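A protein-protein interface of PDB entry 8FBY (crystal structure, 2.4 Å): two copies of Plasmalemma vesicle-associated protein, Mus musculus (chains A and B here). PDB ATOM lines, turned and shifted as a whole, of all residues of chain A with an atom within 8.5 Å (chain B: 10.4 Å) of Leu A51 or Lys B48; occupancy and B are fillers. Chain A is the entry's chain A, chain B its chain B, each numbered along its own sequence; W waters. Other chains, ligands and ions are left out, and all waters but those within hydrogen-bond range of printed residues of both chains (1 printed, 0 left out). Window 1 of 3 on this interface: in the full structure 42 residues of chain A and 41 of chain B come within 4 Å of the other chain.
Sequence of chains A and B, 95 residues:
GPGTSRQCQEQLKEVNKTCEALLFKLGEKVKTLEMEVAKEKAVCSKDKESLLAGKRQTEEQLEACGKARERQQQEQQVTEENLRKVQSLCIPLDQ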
ATOM      1  N   GLU A  40     -19.659 -16.992 -17.751  1.00  0.00           N
ATOM      2  CA  GLU A  40     -19.872 -17.256 -16.332  1.00  0.00           C
ATOM      3  C   GLU A  40     -19.259 -18.592 -15.930  1.00  0.00           C
ATOM      4  O   GLU A  40     -18.582 -18.664 -14.908  1.00  0.00           O
ATOM      5  CB  GLU A  40     -21.357 -17.188 -15.944  1.00  0.00           C
ATOM      6  CG  GLU A  40     -22.069 -15.853 -16.169  1.00  0.00           C
ATOM      7  CD  GLU A  40     -21.781 -14.632 -15.304  1.00  0.00           C
ATOM      8  OE1 GLU A  40     -22.032 -13.506 -15.798  1.00  0.00           O
ATOM      9  OE2 GLU A  40     -21.341 -14.785 -14.139  1.00  0.00           O
ATOM     10  N   ALA A  42     -16.706 -20.166 -17.370  1.00  0.00           N
ATOM     11  CA  ALA A  42     -15.235 -20.012 -17.446  1.00  0.00           C
ATOM     12  C   ALA A  42     -14.646 -19.185 -16.278  1.00  0.00           C
ATOM     13  O   ALA A  42     -13.590 -19.542 -15.752  1.00  0.00           O
ATOM     14  CB  ALA A  42     -14.841 -19.386 -18.783  1.00  0.00           C
ATOM     15  N   VAL A  43     -15.318 -18.084 -15.886  1.00  0.00           N
ATOM     16  CA  VAL A  43     -14.912 -17.223 -14.768  1.00  0.00           C
ATOM     17  C   VAL A  43     -15.106 -17.983 -13.433  1.00  0.00           C
ATOM     18  O   VAL A  43     -14.253 -17.887 -12.549  1.00  0.00           O
ATOM     19  CB  VAL A  43     -15.666 -15.856 -14.790  1.00  0.00           C
ATOM     20  CG1 VAL A  43     -15.324 -14.996 -13.574  1.00  0.00           C
ATOM     21  CG2 VAL A  43     -15.377 -15.084 -16.079  1.00  0.00           C
ATOM     22  N   CYS A  44     -16.207 -18.749 -13.297  1.00  0.00           N
ATOM     23  CA  CYS A  44     -16.483 -19.523 -12.094  1.00  0.00           C
ATOM     24  C   CYS A  44     -15.361 -20.510 -11.816  1.00  0.00           C
ATOM     25  O   CYS A  44     -14.835 -20.522 -10.704  1.00  0.00           O
ATOM     26  CB  CYS A  44     -17.830 -20.236 -12.190  1.00  0.00           C
ATOM     27  SG  CYS A  44     -18.480 -20.784 -10.589  1.00  0.00           S
ATOM     28  N   SER A  45     -15.003 -21.337 -12.822  1.00  0.00           N
ATOM     29  CA  SER A  45     -13.957 -22.354 -12.681  1.00  0.00           C
ATOM     30  C   SER A  45     -12.580 -21.737 -12.391  1.00  0.00           C
ATOM     31  O   SER A  45     -11.850 -22.268 -11.556  1.00  0.00           O
ATOM     32  CB  SER A  45     -13.901 -23.277 -13.899  1.00  0.00           C
ATOM     33  OG  SER A  45     -15.143 -23.893 -14.192  1.00  0.00           O
ATOM     34  N   LYS A  46     -12.267 -20.593 -13.021  1.00  0.00           N
ATOM     35  CA  LYS A  46     -11.018 -19.857 -12.810  1.00  0.00           C
ATOM     36  C   LYS A  46     -10.941 -19.334 -11.369  1.00  0.00           C
ATOM     37  O   LYS A  46      -9.912 -19.507 -10.720  1.00  0.00           O
ATOM     38  CB  LYS A  46     -10.920 -18.698 -13.811  1.00  0.00           C
ATOM     39  CG  LYS A  46      -9.627 -17.892 -13.747  1.00  0.00           C
ATOM     40  CD  LYS A  46      -9.767 -16.599 -14.538  1.00  0.00           C
ATOM     41  CE  LYS A  46      -8.434 -16.006 -14.918  1.00  0.00           C
ATOM     42  NZ  LYS A  46      -7.991 -16.453 -16.272  1.00  0.00           N
ATOM     43  N   ASP A  47     -12.026 -18.713 -10.870  1.00  0.00           N
ATOM     44  CA  ASP A  47     -12.112 -18.177  -9.503  1.00  0.00           C
ATOM     45  C   ASP A  47     -12.011 -19.271  -8.444  1.00  0.00           C
ATOM     46  O   ASP A  47     -11.288 -19.094  -7.456  1.00  0.00           O
ATOM     47  CB  ASP A  47     -13.393 -17.338  -9.315  1.00  0.00           C
ATOM     48  CG  ASP A  47     -13.377 -15.970  -9.987  1.00  0.00           C
ATOM     49  OD1 ASP A  47     -12.363 -15.640 -10.660  1.00  0.00           O
ATOM     50  OD2 ASP A  47     -14.374 -15.223  -9.838  1.00  0.00           O
ATOM     51  N   LYS A  48     -12.702 -20.404  -8.668  1.00  0.00           N
ATOM     52  CA  LYS A  48     -12.681 -21.580  -7.782  1.00  0.00           C
ATOM     53  C   LYS A  48     -11.263 -22.144  -7.661  1.00  0.00           C
ATOM     54  O   LYS A  48     -10.829 -22.444  -6.554  1.00  0.00           O
ATOM     55  CB  LYS A  48     -13.654 -22.664  -8.271  1.00  0.00           C
ATOM     56  CG  LYS A  48     -15.075 -22.509  -7.737  1.00  0.00           C
ATOM     57  CD  LYS A  48     -15.988 -23.616  -8.253  1.00  0.00           C
ATOM     58  CE  LYS A  48     -17.446 -23.278  -8.025  1.00  0.00           C
ATOM     59  NZ  LYS A  48     -18.349 -24.327  -8.566  1.00  0.00           N
ATOM     60  N   GLU A  49     -10.530 -22.237  -8.787  1.00  0.00           N
ATOM     61  CA  GLU A  49      -9.147 -22.720  -8.841  1.00  0.00           C
ATOM     62  C   GLU A  49      -8.199 -21.832  -8.012  1.00  0.00           C
ATOM     63  O   GLU A  49      -7.352 -22.373  -7.299  1.00  0.00           O
ATOM     64  CB  GLU A  49      -8.665 -22.821 -10.305  1.00  0.00           C
ATOM     65  CG  GLU A  49      -7.559 -23.835 -10.530  1.00  0.00           C
ATOM     66  CD  GLU A  49      -6.747 -23.683 -11.807  1.00  0.00           C
ATOM     67  OE1 GLU A  49      -5.517 -23.917 -11.755  1.00  0.00           O
ATOM     68  OE2 GLU A  49      -7.334 -23.330 -12.858  1.00  0.00           O
ATOM     69  N   SER A  50      -8.352 -20.486  -8.089  1.00  0.00           N
ATOM     70  CA  SER A  50      -7.536 -19.539  -7.311  1.00  0.00           C
ATOM     71  C   SER A  50      -7.813 -19.696  -5.805  1.00  0.00           C
ATOM     72  O   SER A  50      -6.872 -19.773  -5.008  1.00  0.00           O
ATOM     73  CB  SER A  50      -7.793 -18.097  -7.747  1.00  0.00           C
ATOM     74  OG  SER A  50      -7.411 -17.869  -9.092  1.00  0.00           O
ATOM     75  N   LEU A  51      -9.102 -19.786  -5.432  1.00  0.00           N
ATOM     76  CA  LEU A  51      -9.531 -19.979  -4.044  1.00  0.00           C
ATOM     77  C   LEU A  51      -9.006 -21.282  -3.463  1.00  0.00           C
ATOM     78  O   LEU A  51      -8.530 -21.277  -2.331  1.00  0.00           O
ATOM     79  CB  LEU A  51     -11.068 -19.906  -3.892  1.00  0.00           C
ATOM     80  CG  LEU A  51     -11.678 -18.518  -3.843  1.00  0.00           C
ATOM     81  CD1 LEU A  51     -13.173 -18.572  -4.101  1.00  0.00           C
ATOM     82  CD2 LEU A  51     -11.389 -17.824  -2.518  1.00  0.00           C
ATOM     83  N   LEU A  52      -9.071 -22.374  -4.239  1.00  0.00           N
ATOM     84  CA  LEU A  52      -8.582 -23.682  -3.812  1.00  0.00           C
ATOM     85  C   LEU A  52      -7.065 -23.699  -3.649  1.00  0.00           C
ATOM     86  O   LEU A  52      -6.586 -24.284  -2.678  1.00  0.00           O
ATOM     87  CB  LEU A  52      -9.055 -24.807  -4.743  1.00  0.00           C
ATOM     88  CG  LEU A  52     -10.463 -25.342  -4.494  1.00  0.00           C
ATOM     89  CD1 LEU A  52     -10.885 -26.221  -5.621  1.00  0.00           C
ATOM     90  CD2 LEU A  52     -10.562 -26.121  -3.173  1.00  0.00           C
ATOM     91  N   ALA A  53      -6.318 -23.020  -4.554  1.00  0.00           N
ATOM     92  CA  ALA A  53      -4.855 -22.915  -4.494  1.00  0.00           C
ATOM     93  C   ALA A  53      -4.403 -22.154  -3.240  1.00  0.00           C
ATOM     94  O   ALA A  53      -3.474 -22.608  -2.545  1.00  0.00           O
ATOM     95  CB  ALA A  53      -4.313 -22.244  -5.745  1.00  0.00           C
ATOM     96  N   GLY A  54      -5.087 -21.033  -2.950  1.00  0.00           N
ATOM     97  CA  GLY A  54      -4.819 -20.218  -1.765  1.00  0.00           C
ATOM     98  C   GLY A  54      -5.075 -20.984  -0.478  1.00  0.00           C
ATOM     99  O   GLY A  54      -4.281 -20.933   0.472  1.00  0.00           O
ATOM    100  N   LYS A  55      -6.187 -21.737  -0.471  1.00  0.00           N
ATOM    101  CA  LYS A  55      -6.623 -22.570   0.647  1.00  0.00           C
ATOM    102  C   LYS A  55      -5.655 -23.742   0.863  1.00  0.00           C
ATOM    103  O   LYS A  55      -5.344 -24.040   2.010  1.00  0.00           O
ATOM    104  CB  LYS A  55      -8.057 -23.062   0.414  1.00  0.00           C
ATOM    105  CG  LYS A  55      -8.714 -23.711   1.617  1.00  0.00           C
ATOM    106  CD  LYS A  55     -10.186 -23.979   1.356  1.00  0.00           C
ATOM    107  CE  LYS A  55     -10.866 -24.509   2.595  1.00  0.00           C
ATOM    108  NZ  LYS A  55     -10.628 -25.957   2.797  1.00  0.00           N
ATOM    109  N   ARG A  56      -5.149 -24.379  -0.223  1.00  0.00           N
ATOM    110  CA  ARG A  56      -4.181 -25.483  -0.120  1.00  0.00           C
ATOM    111  C   ARG A  56      -2.875 -25.016   0.526  1.00  0.00           C
ATOM    112  O   ARG A  56      -2.309 -25.726   1.367  1.00  0.00           O
ATOM    113  CB  ARG A  56      -3.878 -26.082  -1.493  1.00  0.00           C
ATOM    114  CG  ARG A  56      -4.627 -27.381  -1.764  1.00  0.00           C
ATOM    115  CD  ARG A  56      -4.104 -28.134  -2.988  1.00  0.00           C
ATOM    116  NE  ARG A  56      -4.061 -27.313  -4.207  1.00  0.00           N
ATOM    117  CZ  ARG A  56      -5.098 -27.070  -5.011  1.00  0.00           C
ATOM    118  NH1 ARG A  56      -6.299 -27.571  -4.731  1.00  0.00           N
ATOM    119  NH2 ARG A  56      -4.945 -26.317  -6.093  1.00  0.00           N
ATOM    120  N   GLN A  57      -2.414 -23.811   0.148  1.00  0.00           N
ATOM    121  CA  GLN A  57      -1.191 -23.229   0.692  1.00  0.00           C
ATOM    122  C   GLN A  57      -1.318 -22.985   2.216  1.00  0.00           C
ATOM    123  O   GLN A  57      -0.378 -23.273   2.960  1.00  0.00           O
ATOM    124  CB  GLN A  57      -0.834 -21.933  -0.061  1.00  0.00           C
ATOM    125  CG  GLN A  57       0.548 -21.368   0.314  1.00  0.00           C
ATOM    126  CD  GLN A  57       0.657 -19.881   0.063  1.00  0.00           C
ATOM    127  OE1 GLN A  57      -0.085 -19.067   0.632  1.00  0.00           O
ATOM    128  NE2 GLN A  57       1.588 -19.490  -0.791  1.00  0.00           N
ATOM    129  N   THR A  58      -2.485 -22.483   2.670  1.00  0.00           N
ATOM    130  CA  THR A  58      -2.739 -22.220   4.090  1.00  0.00           C
ATOM    131  C   THR A  58      -2.814 -23.519   4.887  1.00  0.00           C
ATOM    132  O   THR A  58      -2.356 -23.555   6.037  1.00  0.00           O
ATOM    133  CB  THR A  58      -3.977 -21.338   4.286  1.00  0.00           C
ATOM    134  OG1 THR A  58      -3.942 -20.260   3.352  1.00  0.00           O
ATOM    135  CG2 THR A  58      -4.082 -20.783   5.696  1.00  0.00           C
ATOM    136  N   GLU A  59      -3.366 -24.588   4.276  1.00  0.00           N
ATOM    137  CA  GLU A  59      -3.475 -25.905   4.910  1.00  0.00           C
ATOM    138  C   GLU A  59      -2.116 -26.539   5.127  1.00  0.00           C
ATOM    139  O   GLU A  59      -1.913 -27.159   6.172  1.00  0.00           O
ATOM    140  CB  GLU A  59      -4.403 -26.833   4.128  1.00  0.00           C
ATOM    141  CG  GLU A  59      -5.868 -26.487   4.339  1.00  0.00           C
ATOM    142  CD  GLU A  59      -6.889 -27.116   3.410  1.00  0.00           C
ATOM    143  OE1 GLU A  59      -6.503 -27.875   2.491  1.00  0.00           O
ATOM    144  OE2 GLU A  59      -8.093 -26.838   3.607  1.00  0.00           O
ATOM    145  N   GLU B  40     -26.999 -20.681 -12.641  1.00  0.00           N
ATOM    146  CA  GLU B  40     -25.544 -20.786 -12.562  1.00  0.00           C
ATOM    147  C   GLU B  40     -24.944 -19.708 -11.648  1.00  0.00           C
ATOM    148  O   GLU B  40     -24.055 -20.011 -10.862  1.00  0.00           O
ATOM    149  CB  GLU B  40     -24.906 -20.811 -13.975  1.00  0.00           C
ATOM    150  CG  GLU B  40     -23.668 -19.938 -14.182  1.00  0.00           C
ATOM    151  CD  GLU B  40     -22.355 -20.377 -13.559  1.00  0.00           C
ATOM    152  OE1 GLU B  40     -22.328 -21.420 -12.863  1.00  0.00           O
ATOM    153  OE2 GLU B  40     -21.340 -19.675 -13.774  1.00  0.00           O
ATOM    154  N   LYS B  41     -25.438 -18.464 -11.734  1.00  0.00           N
ATOM    155  CA  LYS B  41     -24.968 -17.360 -10.896  1.00  0.00           C
ATOM    156  C   LYS B  41     -25.257 -17.625  -9.419  1.00  0.00           C
ATOM    157  O   LYS B  41     -24.408 -17.322  -8.581  1.00  0.00           O
ATOM    158  CB  LYS B  41     -25.574 -16.033 -11.318  1.00  0.00           C
ATOM    159  CG  LYS B  41     -24.991 -15.459 -12.602  1.00  0.00           C
ATOM    160  CD  LYS B  41     -25.691 -14.137 -12.906  1.00  0.00           C
ATOM    161  CE  LYS B  41     -25.060 -13.325 -14.002  1.00  0.00           C
ATOM    162  NZ  LYS B  41     -26.029 -12.327 -14.555  1.00  0.00           N
ATOM    163  N   ALA B  42     -26.410 -18.234  -9.102  1.00  0.00           N
ATOM    164  CA  ALA B  42     -26.777 -18.567  -7.722  1.00  0.00           C
ATOM    165  C   ALA B  42     -25.904 -19.678  -7.155  1.00  0.00           C
ATOM    166  O   ALA B  42     -25.461 -19.540  -6.019  1.00  0.00           O
ATOM    167  CB  ALA B  42     -28.259 -18.919  -7.621  1.00  0.00           C
ATOM    168  N   VAL B  43     -25.637 -20.750  -7.938  1.00  0.00           N
ATOM    169  CA  VAL B  43     -24.797 -21.901  -7.534  1.00  0.00           C
ATOM    170  C   VAL B  43     -23.333 -21.463  -7.373  1.00  0.00           C
ATOM    171  O   VAL B  43     -22.688 -21.826  -6.393  1.00  0.00           O
ATOM    172  CB  VAL B  43     -24.941 -23.102  -8.526  1.00  0.00           C
ATOM    173  CG1 VAL B  43     -23.954 -24.227  -8.190  1.00  0.00           C
ATOM    174  CG2 VAL B  43     -26.364 -23.652  -8.521  1.00  0.00           C
ATOM    175  N   CYS B  44     -22.832 -20.679  -8.335  1.00  0.00           N
ATOM    176  CA  CYS B  44     -21.466 -20.169  -8.333  1.00  0.00           C
ATOM    177  C   CYS B  44     -21.185 -19.290  -7.133  1.00  0.00           C
ATOM    178  O   CYS B  44     -20.197 -19.518  -6.442  1.00  0.00           O
ATOM    179  CB  CYS B  44     -21.142 -19.445  -9.640  1.00  0.00           C
ATOM    180  SG  CYS B  44     -19.374 -19.057  -9.871  1.00  0.00           S
ATOM    181  N   SER B  45     -22.038 -18.295  -6.886  1.00  0.00           N
ATOM    182  CA  SER B  45     -21.814 -17.354  -5.798  1.00  0.00           C
ATOM    183  C   SER B  45     -21.938 -18.017  -4.414  1.00  0.00           C
ATOM    184  O   SER B  45     -21.152 -17.699  -3.524  1.00  0.00           O
ATOM    185  CB  SER B  45     -22.686 -16.118  -5.950  1.00  0.00           C
ATOM    186  OG  SER B  45     -24.049 -16.472  -5.844  1.00  0.00           O
ATOM    187  N   LYS B  46     -22.843 -18.994  -4.269  1.00  0.00           N
ATOM    188  CA  LYS B  46     -23.007 -19.764  -3.038  1.00  0.00           C
ATOM    189  C   LYS B  46     -21.735 -20.594  -2.764  1.00  0.00           C
ATOM    190  O   LYS B  46     -21.242 -20.562  -1.638  1.00  0.00           O
ATOM    191  CB  LYS B  46     -24.233 -20.691  -3.161  1.00  0.00           C
ATOM    192  CG  LYS B  46     -24.535 -21.531  -1.928  1.00  0.00           C
ATOM    193  CD  LYS B  46     -25.560 -22.597  -2.262  1.00  0.00           C
ATOM    194  CE  LYS B  46     -26.412 -22.963  -1.090  1.00  0.00           C
ATOM    195  NZ  LYS B  46     -27.726 -23.456  -1.562  1.00  0.00           N
ATOM    196  N   ASP B  47     -21.212 -21.311  -3.790  1.00  0.00           N
ATOM    197  CA  ASP B  47     -20.004 -22.137  -3.698  1.00  0.00           C
ATOM    198  C   ASP B  47     -18.763 -21.298  -3.393  1.00  0.00           C
ATOM    199  O   ASP B  47     -17.976 -21.693  -2.540  1.00  0.00           O
ATOM    200  CB  ASP B  47     -19.801 -22.982  -4.969  1.00  0.00           C
ATOM    201  CG  ASP B  47     -20.762 -24.155  -5.151  1.00  0.00           C
ATOM    202  OD1 ASP B  47     -21.673 -24.325  -4.304  1.00  0.00           O
ATOM    203  OD2 ASP B  47     -20.602 -24.905  -6.140  1.00  0.00           O
ATOM    204  N   LYS B  48     -18.610 -20.140  -4.051  1.00  0.00           N
ATOM    205  CA  LYS B  48     -17.508 -19.188  -3.835  1.00  0.00           C
ATOM    206  C   LYS B  48     -17.495 -18.681  -2.391  1.00  0.00           C
ATOM    207  O   LYS B  48     -16.421 -18.605  -1.783  1.00  0.00           O
ATOM    208  CB  LYS B  48     -17.597 -17.990  -4.791  1.00  0.00           C
ATOM    209  CG  LYS B  48     -16.876 -18.146  -6.127  1.00  0.00           C
ATOM    210  CD  LYS B  48     -17.036 -16.860  -6.942  1.00  0.00           C
ATOM    211  CE  LYS B  48     -16.791 -17.030  -8.414  1.00  0.00           C
ATOM    212  NZ  LYS B  48     -17.099 -15.787  -9.185  1.00  0.00           N
ATOM    213  N   GLU B  49     -18.685 -18.350  -1.838  1.00  0.00           N
ATOM    214  CA  GLU B  49     -18.840 -17.880  -0.461  1.00  0.00           C
ATOM    215  C   GLU B  49     -18.395 -18.946   0.557  1.00  0.00           C
ATOM    216  O   GLU B  49     -17.726 -18.598   1.537  1.00  0.00           O
ATOM    217  CB  GLU B  49     -20.279 -17.431  -0.173  1.00  0.00           C
ATOM    218  CG  GLU B  49     -20.306 -16.344   0.893  1.00  0.00           C
ATOM    219  CD  GLU B  49     -21.614 -16.072   1.604  1.00  0.00           C
ATOM    220  OE1 GLU B  49     -22.687 -16.247   0.984  1.00  0.00           O
ATOM    221  OE2 GLU B  49     -21.564 -15.662   2.786  1.00  0.00           O
ATOM    222  N   SER B  50     -18.758 -20.230   0.326  1.00  0.00           N
ATOM    223  CA  SER B  50     -18.353 -21.337   1.199  1.00  0.00           C
ATOM    224  C   SER B  50     -16.836 -21.530   1.143  1.00  0.00           C
ATOM    225  O   SER B  50     -16.226 -21.680   2.195  1.00  0.00           O
ATOM    226  CB  SER B  50     -19.064 -22.637   0.835  1.00  0.00           C
ATOM    227  OG  SER B  50     -20.461 -22.532   1.036  1.00  0.00           O
ATOM    228  N   LEU B  51     -16.232 -21.494  -0.065  1.00  0.00           N
ATOM    229  CA  LEU B  51     -14.783 -21.629  -0.250  1.00  0.00           C
ATOM    230  C   LEU B  51     -14.018 -20.504   0.427  1.00  0.00           C
ATOM    231  O   LEU B  51     -12.987 -20.757   1.046  1.00  0.00           O
ATOM    232  CB  LEU B  51     -14.391 -21.721  -1.738  1.00  0.00           C
ATOM    233  CG  LEU B  51     -14.577 -23.082  -2.397  1.00  0.00           C
ATOM    234  CD1 LEU B  51     -14.570 -22.953  -3.912  1.00  0.00           C
ATOM    235  CD2 LEU B  51     -13.520 -24.059  -1.961  1.00  0.00           C
ATOM    236  N   LEU B  52     -14.518 -19.263   0.320  1.00  0.00           N
ATOM    237  CA  LEU B  52     -13.884 -18.107   0.945  1.00  0.00           C
ATOM    238  C   LEU B  52     -13.995 -18.178   2.480  1.00  0.00           C
ATOM    239  O   LEU B  52     -13.013 -17.887   3.161  1.00  0.00           O
ATOM    240  CB  LEU B  52     -14.447 -16.779   0.371  1.00  0.00           C
ATOM    241  CG  LEU B  52     -13.806 -15.459   0.856  1.00  0.00           C
ATOM    242  CD1 LEU B  52     -12.344 -15.331   0.420  1.00  0.00           C
ATOM    243  CD2 LEU B  52     -14.566 -14.263   0.352  1.00  0.00           C
ATOM    244  N   ALA B  53     -15.154 -18.622   3.015  1.00  0.00           N
ATOM    245  CA  ALA B  53     -15.378 -18.790   4.464  1.00  0.00           C
ATOM    246  C   ALA B  53     -14.488 -19.890   5.031  1.00  0.00           C
ATOM    247  O   ALA B  53     -13.916 -19.690   6.094  1.00  0.00           O
ATOM    248  CB  ALA B  53     -16.833 -19.102   4.758  1.00  0.00           C
ATOM    249  N   GLY B  54     -14.358 -21.008   4.311  1.00  0.00           N
ATOM    250  CA  GLY B  54     -13.494 -22.131   4.663  1.00  0.00           C
ATOM    251  C   GLY B  54     -12.032 -21.720   4.698  1.00  0.00           C
ATOM    252  O   GLY B  54     -11.313 -22.104   5.616  1.00  0.00           O
ATOM    253  N   LYS B  55     -11.601 -20.895   3.729  1.00  0.00           N
ATOM    254  CA  LYS B  55     -10.243 -20.358   3.636  1.00  0.00           C
ATOM    255  C   LYS B  55      -9.964 -19.434   4.828  1.00  0.00           C
ATOM    256  O   LYS B  55      -8.884 -19.505   5.413  1.00  0.00           O
ATOM    257  CB  LYS B  55     -10.051 -19.620   2.298  1.00  0.00           C
ATOM    258  CG  LYS B  55      -8.649 -19.071   2.047  1.00  0.00           C
ATOM    259  CD  LYS B  55      -8.484 -18.637   0.598  1.00  0.00           C
ATOM    260  CE  LYS B  55      -7.876 -17.270   0.324  1.00  0.00           C
ATOM    261  NZ  LYS B  55      -6.512 -17.115   0.905  1.00  0.00           N
ATOM    262  N   ARG B  56     -10.938 -18.573   5.180  1.00  0.00           N
ATOM    263  CA  ARG B  56     -10.856 -17.631   6.297  1.00  0.00           C
ATOM    264  C   ARG B  56     -10.741 -18.325   7.655  1.00  0.00           C
ATOM    265  O   ARG B  56     -10.027 -17.831   8.527  1.00  0.00           O
ATOM    266  CB  ARG B  56     -12.034 -16.645   6.250  1.00  0.00           C
ATOM    267  CG  ARG B  56     -11.627 -15.180   6.456  1.00  0.00           C
ATOM    268  CD  ARG B  56     -10.695 -14.632   5.377  1.00  0.00           C
ATOM    269  NE  ARG B  56     -11.418 -13.755   4.466  1.00  0.00           N
ATOM    270  CZ  ARG B  56     -10.990 -13.391   3.262  1.00  0.00           C
ATOM    271  NH1 ARG B  56      -9.822 -13.837   2.800  1.00  0.00           N
ATOM    272  NH2 ARG B  56     -11.730 -12.590   2.502  1.00  0.00           N
ATOM    273  N   THR B  58      -9.362 -21.480   8.084  1.00  0.00           N
ATOM    274  CA  THR B  58      -8.027 -22.125   8.109  1.00  0.00           C
ATOM    275  C   THR B  58      -6.955 -21.079   8.429  1.00  0.00           C
ATOM    276  O   THR B  58      -6.018 -21.411   9.150  1.00  0.00           O
ATOM    277  CB  THR B  58      -7.776 -22.900   6.811  1.00  0.00           C
ATOM    278  OG1 THR B  58      -8.905 -23.736   6.570  1.00  0.00           O
ATOM    279  CG2 THR B  58      -6.523 -23.744   6.851  1.00  0.00           C
ATOM    280  N   GLU B  59      -7.105 -19.861   7.922  1.00  0.00           N
ATOM    281  CA  GLU B  59      -6.147 -18.769   8.218  1.00  0.00           C
ATOM    282  C   GLU B  59      -6.184 -18.434   9.710  1.00  0.00           C
ATOM    283  O   GLU B  59      -5.116 -18.181  10.259  1.00  0.00           O
ATOM    284  CB  GLU B  59      -6.509 -17.542   7.388  1.00  0.00           C
ATOM    285  CG  GLU B  59      -6.063 -17.618   5.944  1.00  0.00           C
ATOM    286  CD  GLU B  59      -6.654 -16.543   5.050  1.00  0.00           C
ATOM    287  OE1 GLU B  59      -7.390 -15.686   5.568  1.00  0.00           O
ATOM    288  OE2 GLU B  59      -6.372 -16.565   3.842  1.00  0.00           O
HETATM  289  O   HOH W   1     -21.475 -16.929 -12.546  1.00  0.00           O
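The side-chain sulfur (SG) of Cys B44 forms a disulfide with the side-chain sulfur (SG) of Cys A44 (2.1 Å).
The side-chain carboxylate (OD2) of Asp A47 is in salt-bridge range of the side-chain amino group (NZ) of Lys B48, 2.9 Å away.
The side-chain amino group (NZ) of Lys A48 lies within salt-bridge range of the side-chain carboxylate (OD2) of Asp B47 (3.4 Å).
The backbone carbonyl oxygen (O) of Glu A40 sits close to the side-chain carboxylate (OE2) of Glu B40 (3.1 Å).
O of Gly A54 sits at hydrogen-bond distance from OG1 of Thr A58, at 3.0 Å.
The side-chain amino group (NZ) of Lys A55 is in salt-bridge range of the side-chain carboxylate (OE2) of Glu A59 (2.8 Å).
The backbone carbonyl oxygen (O) of Lys B41 sits at hydrogen-bond distance from the side-chain hydroxyl (OG) of Ser B45, at 2.9 Å.
O of Gly B54 sits at hydrogen-bond distance from OG1 of Thr B58 (3.1 Å).
The side-chain carboxylate of Glu B59 is in salt-bridge range of the side-chain amino group of Lys B55 (3.0 Å).
Glu A40 touches Lys B41 (OE1 to CE, 3.5 Å).
Leu B51 touches Lys A48.
Leu A51 touches Lys B48 (CD1 to O, 3.99 Å).
CD1 of Leu B52 touches CD2 of Leu A51, 3.97 Å away.
Leu A51 touches Lys B55.
Leu A52 touches Leu B51.
Lys A55 touches Gly B54 (CE to C, 3.7 Å).
N of Lys B55 touches CE of Lys A55, 3.9 Å away.
Thr B58 touches Thr A58 (C to CG2, 3.98 Å).
Thr A58 touches Glu B59.
Of the printed residues of chain A, Lys B48 touches Asp A47 (2.9 Å) and Leu A51 (3.99 Å).
Of chain B, only Asp B47 and Leu B51 come within 4 Å of Lys A48.
Ser A50 touches none of the printed residues of chain B.
Of chain B, only Leu B51 (3.8 Å) comes within 4 Å of Leu A52.
Ala A53 touches none of the printed residues of chain B.
Printed residues of chain A within 4 Å of Cys B44: Cys A44 (2.1 Å).
Of the printed residues of chain B, Lys A55 touches Gly B54 and Lys B55.
Arg B56 touches none of the printed residues of chain A.
The nearest printed residue of chain B that does not touch Glu A59 is Gly B54 (6.1 Å).
Of the 19 printed residues of chain B, 11 touch a printed residue of chain A.
Hydrophobic or aromatic side chains of chain B that line the printed part of chain A: Leu B51 and Leu B52.
Along chain B the printed residues that touch a printed residue of chain A span positions 40 to 59.
Printed residues of chain A that touch a printed residue of chain B: Glu A40, Cys A44, Asp A47, Lys A48, Leu A51, Leu A52, Lys A55, Thr A58 and Glu A59.
Among the printed residues, 16 pairs touch across the chains.
Among the printed residues, Asp or Glu carboxylates within 4 Å of a Lys or Arg side-chain nitrogen of the other chain: Asp A47 with Lys B48 and Lys A48 with Asp B47.
Cys A44 touches its own counterpart, Cys B44.
Asp A47 touches Lys B48, and with the chains exchanged Lys A48 touches Asp B47.
Lys B55 touches its own counterpart, Lys A55.
Thr B58 touches its own counterpart, Thr A58.
Positions printed for both chains: 40, 42, 43, 44, 45, 46, 47, 48, 49, 50, 51, 52, 53, 54, 55, 56, 58 and 59.
Of the 16 pairs that touch across the chains among the printed residues, 12 have their exchanged pair printed and touching as well.
Water W1 lies within hydrogen-bond range of OE2 of Glu A40 and OE2 of Glu B40.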
